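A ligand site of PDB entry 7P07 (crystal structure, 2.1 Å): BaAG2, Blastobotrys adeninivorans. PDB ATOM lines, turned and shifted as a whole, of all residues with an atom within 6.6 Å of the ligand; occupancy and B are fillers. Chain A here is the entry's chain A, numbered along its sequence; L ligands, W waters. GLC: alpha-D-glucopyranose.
An oxygen (O2) of the ligand is in hydrogen-bond range of a ring nitrogen (NE2) of His 347.
The side-chain carboxylate (OD2) of Asp 71 lies within hydrogen-bond range of an oxygen (O4) of the ligand (2.8 Å).
An oxygen (O6) of the ligand lies within hydrogen-bond range of a ring nitrogen (NE2) of His 114 (3.0 Å).
An oxygen (O1) of the ligand sits at hydrogen-bond distance from the side-chain carboxylate (OE1) of Glu 274 (2.5 Å).
The guanidinium group of Arg 214 lies within hydrogen-bond range of an oxygen (O2) of the ligand, 3.1 Å away.
An oxygen (O4) of the ligand is in hydrogen-bond range of the guanidinium group (NH1) of Arg 440, 2.9 Å away.
The side-chain carboxylate (OD1) of Asp 348 lies within hydrogen-bond range of an oxygen (O3) of the ligand, 2.7 Å away.
The side-chain carboxylate of Glu 274 lies within salt-bridge range of the guanidinium group of Arg 214, at 3.3 Å.
N of Thr 217 sits at hydrogen-bond distance from OE1 of Glu 274 (3.1 Å).
The guanidinium group (NE) of Arg 444 sits at hydrogen-bond distance from the backbone carbonyl oxygen (O) of His 347 (3.1 Å).
The side-chain amide nitrogen (NE2) of Gln 183 lies within hydrogen-bond range of the side-chain carboxylate (OD2) of Asp 71, at 3.1 Å.
The guanidinium group (NH2) of Arg 444 is in salt-bridge range of the side-chain carboxylate (OD1) of Asp 348.
NH2 of Arg 440 lies within salt-bridge range of OD1 of Asp 71 (3.1 Å).
The side-chain hydroxyl of Tyr 74 lies within hydrogen-bond range of a ring nitrogen (NE2) of His 347, 3.1 Å away.
NE2 of His 347 sits close to OD1 of Asp 348 (3.4 Å).
Merely in contact with the ligand: Tyr 74, Phe 160, Phe 179, Gln 183, Asp 216 and Thr 217.
Hydrophobic or aromatic side chains that line the ligand: Tyr 74, His 114, Phe 160, Phe 179 and His 347.
13 residues have an atom within 4 Å of the ligand: Asp 71, Tyr 74, His 114, Phe 160, Phe 179, Gln 183, Arg 214, Asp 216, Thr 217, Glu 274, His 347, Asp 348 and Arg 440.
Water W1 lies within hydrogen-bond range of an oxygen (O3) of the ligand (2.7 Å), the side-chain carboxylate (OD1) of Asp 71 (3.0 Å), the guanidinium group (NH2) of Arg 444 (3.0 Å) and the guanidinium group (NH2) of Arg 440 (3.2 Å).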
ATOM      1  N   TRP A  60      10.633 -14.062 -13.264  1.00  0.00           N
ATOM      2  CA  TRP A  60      11.066 -13.260 -12.102  1.00  0.00           C
ATOM      3  C   TRP A  60      10.135 -12.057 -12.035  1.00  0.00           C
ATOM      4  O   TRP A  60      10.273 -11.225 -12.897  1.00  0.00           O
ATOM      5  CB  TRP A  60      12.536 -12.847 -12.190  1.00  0.00           C
ATOM      6  CG  TRP A  60      12.900 -11.664 -11.348  1.00  0.00           C
ATOM      7  CD1 TRP A  60      12.259 -11.234 -10.223  1.00  0.00           C
ATOM      8  CD2 TRP A  60      13.971 -10.738 -11.567  1.00  0.00           C
ATOM      9  NE1 TRP A  60      12.863 -10.115  -9.742  1.00  0.00           N
ATOM     10  CE2 TRP A  60      13.918  -9.783 -10.536  1.00  0.00           C
ATOM     11  CE3 TRP A  60      14.972 -10.622 -12.528  1.00  0.00           C
ATOM     12  CZ2 TRP A  60      14.809  -8.723 -10.443  1.00  0.00           C
ATOM     13  CZ3 TRP A  60      15.860  -9.575 -12.431  1.00  0.00           C
ATOM     14  CH2 TRP A  60      15.783  -8.647 -11.407  1.00  0.00           C
ATOM     15  N   ASP A  71       9.847   4.314  -4.886  1.00  0.00           N
ATOM     16  CA  ASP A  71      10.870   3.545  -5.625  1.00  0.00           C
ATOM     17  C   ASP A  71      10.174   2.362  -6.319  1.00  0.00           C
ATOM     18  O   ASP A  71      10.736   1.285  -6.366  1.00  0.00           O
ATOM     19  CB  ASP A  71      12.001   3.076  -4.704  1.00  0.00           C
ATOM     20  CG  ASP A  71      13.260   2.642  -5.455  1.00  0.00           C
ATOM     21  OD1 ASP A  71      13.381   2.949  -6.605  1.00  0.00           O
ATOM     22  OD2 ASP A  71      14.084   2.008  -4.843  1.00  0.00           O
ATOM     23  N   TYR A  74      10.038  -1.132  -4.516  1.00  0.00           N
ATOM     24  CA  TYR A  74      11.225  -1.451  -3.684  1.00  0.00           C
ATOM     25  C   TYR A  74      11.152  -0.767  -2.307  1.00  0.00           C
ATOM     26  O   TYR A  74      12.094  -0.923  -1.540  1.00  0.00           O
ATOM     27  CB  TYR A  74      12.494  -1.223  -4.505  1.00  0.00           C
ATOM     28  CG  TYR A  74      12.724  -2.293  -5.547  1.00  0.00           C
ATOM     29  CD1 TYR A  74      13.223  -3.513  -5.178  1.00  0.00           C
ATOM     30  CD2 TYR A  74      12.383  -2.113  -6.864  1.00  0.00           C
ATOM     31  CE1 TYR A  74      13.420  -4.528  -6.092  1.00  0.00           C
ATOM     32  CE2 TYR A  74      12.580  -3.106  -7.805  1.00  0.00           C
ATOM     33  CZ  TYR A  74      13.098  -4.326  -7.421  1.00  0.00           C
ATOM     34  OH  TYR A  74      13.277  -5.304  -8.327  1.00  0.00           O
ATOM     35  N   ASP A  75      10.102   0.005  -2.027  1.00  0.00           N
ATOM     36  CA  ASP A  75       9.801   0.604  -0.703  1.00  0.00           C
ATOM     37  C   ASP A  75       8.533  -0.118  -0.249  1.00  0.00           C
ATOM     38  O   ASP A  75       7.502   0.351  -0.585  1.00  0.00           O
ATOM     39  CB  ASP A  75       9.543   2.087  -0.829  1.00  0.00           C
ATOM     40  CG  ASP A  75       8.583   2.421  -1.928  1.00  0.00           C
ATOM     41  OD1 ASP A  75       8.625   1.742  -2.926  1.00  0.00           O
ATOM     42  OD2 ASP A  75       7.850   3.383  -1.804  1.00  0.00           O
ATOM     43  N   ASP A 109      10.558 -10.919  -5.639  1.00  0.00           N
ATOM     44  CA  ASP A 109      11.675 -10.027  -5.268  1.00  0.00           C
ATOM     45  C   ASP A 109      11.727  -9.954  -3.740  1.00  0.00           C
ATOM     46  O   ASP A 109      10.707  -9.660  -3.189  1.00  0.00           O
ATOM     47  CB  ASP A 109      11.487  -8.671  -5.919  1.00  0.00           C
ATOM     48  CG  ASP A 109      12.699  -8.206  -6.670  1.00  0.00           C
ATOM     49  OD1 ASP A 109      13.739  -8.392  -6.179  1.00  0.00           O
ATOM     50  OD2 ASP A 109      12.578  -7.670  -7.750  1.00  0.00           O
ATOM     51  N   VAL A 111      13.074  -7.811  -0.867  1.00  0.00           N
ATOM     52  CA  VAL A 111      13.632  -6.477  -0.499  1.00  0.00           C
ATOM     53  C   VAL A 111      13.721  -6.370   1.019  1.00  0.00           C
ATOM     54  O   VAL A 111      12.740  -5.946   1.600  1.00  0.00           O
ATOM     55  CB  VAL A 111      12.691  -5.407  -1.048  1.00  0.00           C
ATOM     56  CG1 VAL A 111      13.343  -4.053  -1.131  1.00  0.00           C
ATOM     57  CG2 VAL A 111      12.111  -5.835  -2.383  1.00  0.00           C
ATOM     58  N   HIS A 114      15.907  -2.590   3.554  1.00  0.00           N
ATOM     59  CA  HIS A 114      15.055  -1.466   3.994  1.00  0.00           C
ATOM     60  C   HIS A 114      13.574  -1.779   3.746  1.00  0.00           C
ATOM     61  O   HIS A 114      13.267  -2.678   2.978  1.00  0.00           O
ATOM     62  CB  HIS A 114      15.458  -0.245   3.194  1.00  0.00           C
ATOM     63  CG  HIS A 114      15.451  -0.475   1.721  1.00  0.00           C
ATOM     64  ND1 HIS A 114      16.528  -0.984   1.073  1.00  0.00           N
ATOM     65  CD2 HIS A 114      14.518  -0.237   0.789  1.00  0.00           C
ATOM     66  CE1 HIS A 114      16.256  -1.066  -0.192  1.00  0.00           C
ATOM     67  NE2 HIS A 114      15.047  -0.609  -0.388  1.00  0.00           N
ATOM     68  N   PHE A 160      20.414   7.651  -4.243  1.00  0.00           N
ATOM     69  CA  PHE A 160      19.530   8.598  -4.955  1.00  0.00           C
ATOM     70  C   PHE A 160      19.892  10.046  -4.613  1.00  0.00           C
ATOM     71  O   PHE A 160      19.066  10.877  -4.914  1.00  0.00           O
ATOM     72  CB  PHE A 160      18.063   8.289  -4.633  1.00  0.00           C
ATOM     73  CG  PHE A 160      17.592   6.924  -5.067  1.00  0.00           C
ATOM     74  CD1 PHE A 160      18.227   6.247  -6.096  1.00  0.00           C
ATOM     75  CD2 PHE A 160      16.533   6.313  -4.441  1.00  0.00           C
ATOM     76  CE1 PHE A 160      17.787   4.997  -6.482  1.00  0.00           C
ATOM     77  CE2 PHE A 160      16.090   5.061  -4.836  1.00  0.00           C
ATOM     78  CZ  PHE A 160      16.725   4.407  -5.861  1.00  0.00           C
ATOM     79  N   PHE A 179      19.007   4.301   0.321  1.00  0.00           N
ATOM     80  CA  PHE A 179      18.214   4.628  -0.888  1.00  0.00           C
ATOM     81  C   PHE A 179      17.388   5.904  -0.593  1.00  0.00           C
ATOM     82  O   PHE A 179      17.982   6.819  -0.047  1.00  0.00           O
ATOM     83  CB  PHE A 179      17.576   3.334  -1.369  1.00  0.00           C
ATOM     84  CG  PHE A 179      18.580   2.327  -1.846  1.00  0.00           C
ATOM     85  CD1 PHE A 179      19.107   2.411  -3.113  1.00  0.00           C
ATOM     86  CD2 PHE A 179      19.060   1.360  -1.001  1.00  0.00           C
ATOM     87  CE1 PHE A 179      20.067   1.520  -3.539  1.00  0.00           C
ATOM     88  CE2 PHE A 179      20.014   0.453  -1.431  1.00  0.00           C
ATOM     89  CZ  PHE A 179      20.523   0.548  -2.696  1.00  0.00           C
ATOM     90  N   GLN A 183      12.885   5.090   2.434  1.00  0.00           N
ATOM     91  CA  GLN A 183      13.315   3.677   2.506  1.00  0.00           C
ATOM     92  C   GLN A 183      14.252   3.545   3.703  1.00  0.00           C
ATOM     93  O   GLN A 183      15.399   3.246   3.479  1.00  0.00           O
ATOM     94  CB  GLN A 183      13.959   3.254   1.193  1.00  0.00           C
ATOM     95  CG  GLN A 183      12.940   3.091   0.086  1.00  0.00           C
ATOM     96  CD  GLN A 183      13.553   2.989  -1.285  1.00  0.00           C
ATOM     97  OE1 GLN A 183      14.040   3.954  -1.844  1.00  0.00           O
ATOM     98  NE2 GLN A 183      13.469   1.800  -1.852  1.00  0.00           N
ATOM     99  N   ARG A 214      14.613 -13.180  -5.805  1.00  0.00           N
ATOM    100  CA  ARG A 214      15.653 -12.272  -6.313  1.00  0.00           C
ATOM    101  C   ARG A 214      16.015 -11.429  -5.093  1.00  0.00           C
ATOM    102  O   ARG A 214      15.203 -10.625  -4.730  1.00  0.00           O
ATOM    103  CB  ARG A 214      15.161 -11.488  -7.533  1.00  0.00           C
ATOM    104  CG  ARG A 214      16.201 -10.596  -8.189  1.00  0.00           C
ATOM    105  CD  ARG A 214      16.552  -9.363  -7.388  1.00  0.00           C
ATOM    106  NE  ARG A 214      17.194  -8.370  -8.214  1.00  0.00           N
ATOM    107  CZ  ARG A 214      17.200  -7.076  -7.960  1.00  0.00           C
ATOM    108  NH1 ARG A 214      16.564  -6.622  -6.898  1.00  0.00           N
ATOM    109  NH2 ARG A 214      17.805  -6.247  -8.777  1.00  0.00           N
ATOM    110  N   ILE A 215      17.109 -11.717  -4.411  1.00  0.00           N
ATOM    111  CA  ILE A 215      17.513 -11.013  -3.171  1.00  0.00           C
ATOM    112  C   ILE A 215      18.136  -9.663  -3.525  1.00  0.00           C
ATOM    113  O   ILE A 215      19.218  -9.683  -4.078  1.00  0.00           O
ATOM    114  CB  ILE A 215      18.452 -11.923  -2.379  1.00  0.00           C
ATOM    115  CG1 ILE A 215      17.870 -13.328  -2.319  1.00  0.00           C
ATOM    116  CG2 ILE A 215      18.733 -11.349  -1.010  1.00  0.00           C
ATOM    117  CD1 ILE A 215      18.383 -14.160  -1.192  1.00  0.00           C
ATOM    118  N   ASP A 216      17.509  -8.534  -3.186  1.00  0.00           N
ATOM    119  CA  ASP A 216      18.061  -7.190  -3.460  1.00  0.00           C
ATOM    120  C   ASP A 216      19.268  -6.919  -2.585  1.00  0.00           C
ATOM    121  O   ASP A 216      19.263  -7.449  -1.496  1.00  0.00           O
ATOM    122  CB  ASP A 216      17.128  -6.070  -3.035  1.00  0.00           C
ATOM    123  CG  ASP A 216      15.783  -6.218  -3.653  1.00  0.00           C
ATOM    124  OD1 ASP A 216      15.488  -7.341  -4.001  1.00  0.00           O
ATOM    125  OD2 ASP A 216      15.073  -5.227  -3.805  1.00  0.00           O
ATOM    126  N   THR A 217      20.183  -6.051  -3.062  1.00  0.00           N
ATOM    127  CA  THR A 217      21.371  -5.516  -2.366  1.00  0.00           C
ATOM    128  C   THR A 217      21.888  -6.527  -1.371  1.00  0.00           C
ATOM    129  O   THR A 217      22.005  -6.180  -0.226  1.00  0.00           O
ATOM    130  CB  THR A 217      20.926  -4.238  -1.660  1.00  0.00           C
ATOM    131  OG1 THR A 217      20.195  -4.651  -0.512  1.00  0.00           O
ATOM    132  CG2 THR A 217      20.031  -3.385  -2.507  1.00  0.00           C
ATOM    133  N   GLU A 274      21.597  -9.755  -5.892  1.00  0.00           N
ATOM    134  CA  GLU A 274      21.940  -8.545  -6.647  1.00  0.00           C
ATOM    135  C   GLU A 274      23.219  -7.957  -6.061  1.00  0.00           C
ATOM    136  O   GLU A 274      23.206  -7.608  -4.893  1.00  0.00           O
ATOM    137  CB  GLU A 274      20.808  -7.539  -6.636  1.00  0.00           C
ATOM    138  CG  GLU A 274      20.984  -6.429  -7.645  1.00  0.00           C
ATOM    139  CD  GLU A 274      20.486  -5.085  -7.144  1.00  0.00           C
ATOM    140  OE1 GLU A 274      20.316  -4.962  -5.953  1.00  0.00           O
ATOM    141  OE2 GLU A 274      20.255  -4.209  -7.955  1.00  0.00           O
ATOM    142  N   PHE A 300      27.542  -6.219 -11.124  1.00  0.00           N
ATOM    143  CA  PHE A 300      27.363  -4.917 -11.798  1.00  0.00           C
ATOM    144  C   PHE A 300      28.529  -4.665 -12.773  1.00  0.00           C
ATOM    145  O   PHE A 300      28.376  -3.750 -13.534  1.00  0.00           O
ATOM    146  CB  PHE A 300      27.315  -3.783 -10.769  1.00  0.00           C
ATOM    147  CG  PHE A 300      26.271  -3.910  -9.703  1.00  0.00           C
ATOM    148  CD1 PHE A 300      24.937  -4.017 -10.020  1.00  0.00           C
ATOM    149  CD2 PHE A 300      26.613  -3.865  -8.366  1.00  0.00           C
ATOM    150  CE1 PHE A 300      23.980  -4.105  -9.038  1.00  0.00           C
ATOM    151  CE2 PHE A 300      25.654  -3.942  -7.375  1.00  0.00           C
ATOM    152  CZ  PHE A 300      24.335  -4.053  -7.717  1.00  0.00           C
ATOM    153  N   HIS A 347      15.309  -4.023 -14.888  1.00  0.00           N
ATOM    154  CA  HIS A 347      14.530  -2.802 -14.617  1.00  0.00           C
ATOM    155  C   HIS A 347      15.429  -1.610 -14.245  1.00  0.00           C
ATOM    156  O   HIS A 347      14.925  -0.523 -14.275  1.00  0.00           O
ATOM    157  CB  HIS A 347      13.517  -3.062 -13.496  1.00  0.00           C
ATOM    158  CG  HIS A 347      14.153  -3.424 -12.214  1.00  0.00           C
ATOM    159  ND1 HIS A 347      14.819  -4.594 -12.035  1.00  0.00           N
ATOM    160  CD2 HIS A 347      14.232  -2.782 -11.042  1.00  0.00           C
ATOM    161  CE1 HIS A 347      15.291  -4.649 -10.815  1.00  0.00           C
ATOM    162  NE2 HIS A 347      14.948  -3.558 -10.206  1.00  0.00           N
ATOM    163  N   ASP A 348      16.672  -1.839 -13.856  1.00  0.00           N
ATOM    164  CA  ASP A 348      17.614  -0.772 -13.446  1.00  0.00           C
ATOM    165  C   ASP A 348      18.626  -0.370 -14.525  1.00  0.00           C
ATOM    166  O   ASP A 348      19.607   0.214 -14.161  1.00  0.00           O
ATOM    167  CB  ASP A 348      18.481  -1.230 -12.274  1.00  0.00           C
ATOM    168  CG  ASP A 348      17.726  -1.407 -10.992  1.00  0.00           C
ATOM    169  OD1 ASP A 348      16.722  -0.776 -10.845  1.00  0.00           O
ATOM    170  OD2 ASP A 348      18.182  -2.155 -10.160  1.00  0.00           O
ATOM    171  N   VAL A 408      12.440   8.020  -9.872  1.00  0.00           N
ATOM    172  CA  VAL A 408      12.931   8.879  -8.755  1.00  0.00           C
ATOM    173  C   VAL A 408      14.445   9.106  -8.878  1.00  0.00           C
ATOM    174  O   VAL A 408      14.915  10.130  -8.424  1.00  0.00           O
ATOM    175  CB  VAL A 408      12.638   8.262  -7.382  1.00  0.00           C
ATOM    176  CG1 VAL A 408      13.079   6.820  -7.297  1.00  0.00           C
ATOM    177  CG2 VAL A 408      13.278   9.061  -6.269  1.00  0.00           C
ATOM    178  N   ARG A 440      17.204   4.331 -15.753  1.00  0.00           N
ATOM    179  CA  ARG A 440      16.354   3.144 -15.481  1.00  0.00           C
ATOM    180  C   ARG A 440      15.047   3.262 -16.265  1.00  0.00           C
ATOM    181  O   ARG A 440      14.454   2.238 -16.556  1.00  0.00           O
ATOM    182  CB  ARG A 440      16.179   3.017 -13.966  1.00  0.00           C
ATOM    183  CG  ARG A 440      17.501   2.990 -13.220  1.00  0.00           C
ATOM    184  CD  ARG A 440      17.474   2.671 -11.741  1.00  0.00           C
ATOM    185  NE  ARG A 440      16.326   3.150 -11.018  1.00  0.00           N
ATOM    186  CZ  ARG A 440      16.155   2.982  -9.722  1.00  0.00           C
ATOM    187  NH1 ARG A 440      17.042   2.296  -9.022  1.00  0.00           N
ATOM    188  NH2 ARG A 440      15.106   3.495  -9.118  1.00  0.00           N
ATOM    189  N   ARG A 444      11.472   0.910 -18.284  1.00  0.00           N
ATOM    190  CA  ARG A 444      10.131   0.983 -17.676  1.00  0.00           C
ATOM    191  C   ARG A 444       9.073   1.471 -18.659  1.00  0.00           C
ATOM    192  O   ARG A 444       7.925   1.480 -18.276  1.00  0.00           O
ATOM    193  CB  ARG A 444      10.260   1.812 -16.405  1.00  0.00           C
ATOM    194  CG  ARG A 444      11.260   1.193 -15.445  1.00  0.00           C
ATOM    195  CD  ARG A 444      11.627   2.060 -14.287  1.00  0.00           C
ATOM    196  NE  ARG A 444      12.561   1.349 -13.444  1.00  0.00           N
ATOM    197  CZ  ARG A 444      12.858   1.692 -12.219  1.00  0.00           C
ATOM    198  NH1 ARG A 444      12.273   2.748 -11.681  1.00  0.00           N
ATOM    199  NH2 ARG A 444      13.714   0.987 -11.525  1.00  0.00           N
HETATM  200  C1  GLC L   1      17.132  -2.754  -5.553  1.00  0.00           C
HETATM  201  C2  GLC L   1      16.481  -2.556  -6.909  1.00  0.00           C
HETATM  202  C3  GLC L   1      16.532  -1.151  -7.351  1.00  0.00           C
HETATM  203  C4  GLC L   1      16.053  -0.303  -6.211  1.00  0.00           C
HETATM  204  C5  GLC L   1      17.025  -0.345  -5.091  1.00  0.00           C
HETATM  205  C6  GLC L   1      16.391   0.036  -3.782  1.00  0.00           C
HETATM  206  O1  GLC L   1      18.184  -3.693  -5.618  1.00  0.00           O
HETATM  207  O2  GLC L   1      16.983  -3.386  -7.931  1.00  0.00           O
HETATM  208  O3  GLC L   1      15.659  -1.069  -8.428  1.00  0.00           O
HETATM  209  O4  GLC L   1      15.946   1.016  -6.642  1.00  0.00           O
HETATM  210  O5  GLC L   1      17.600  -1.607  -4.901  1.00  0.00           O
HETATM  211  O6  GLC L   1      15.551  -1.009  -3.342  1.00  0.00           O
HETATM  212  O   HOH W   1      13.675   0.711  -8.531  1.00  0.00           O
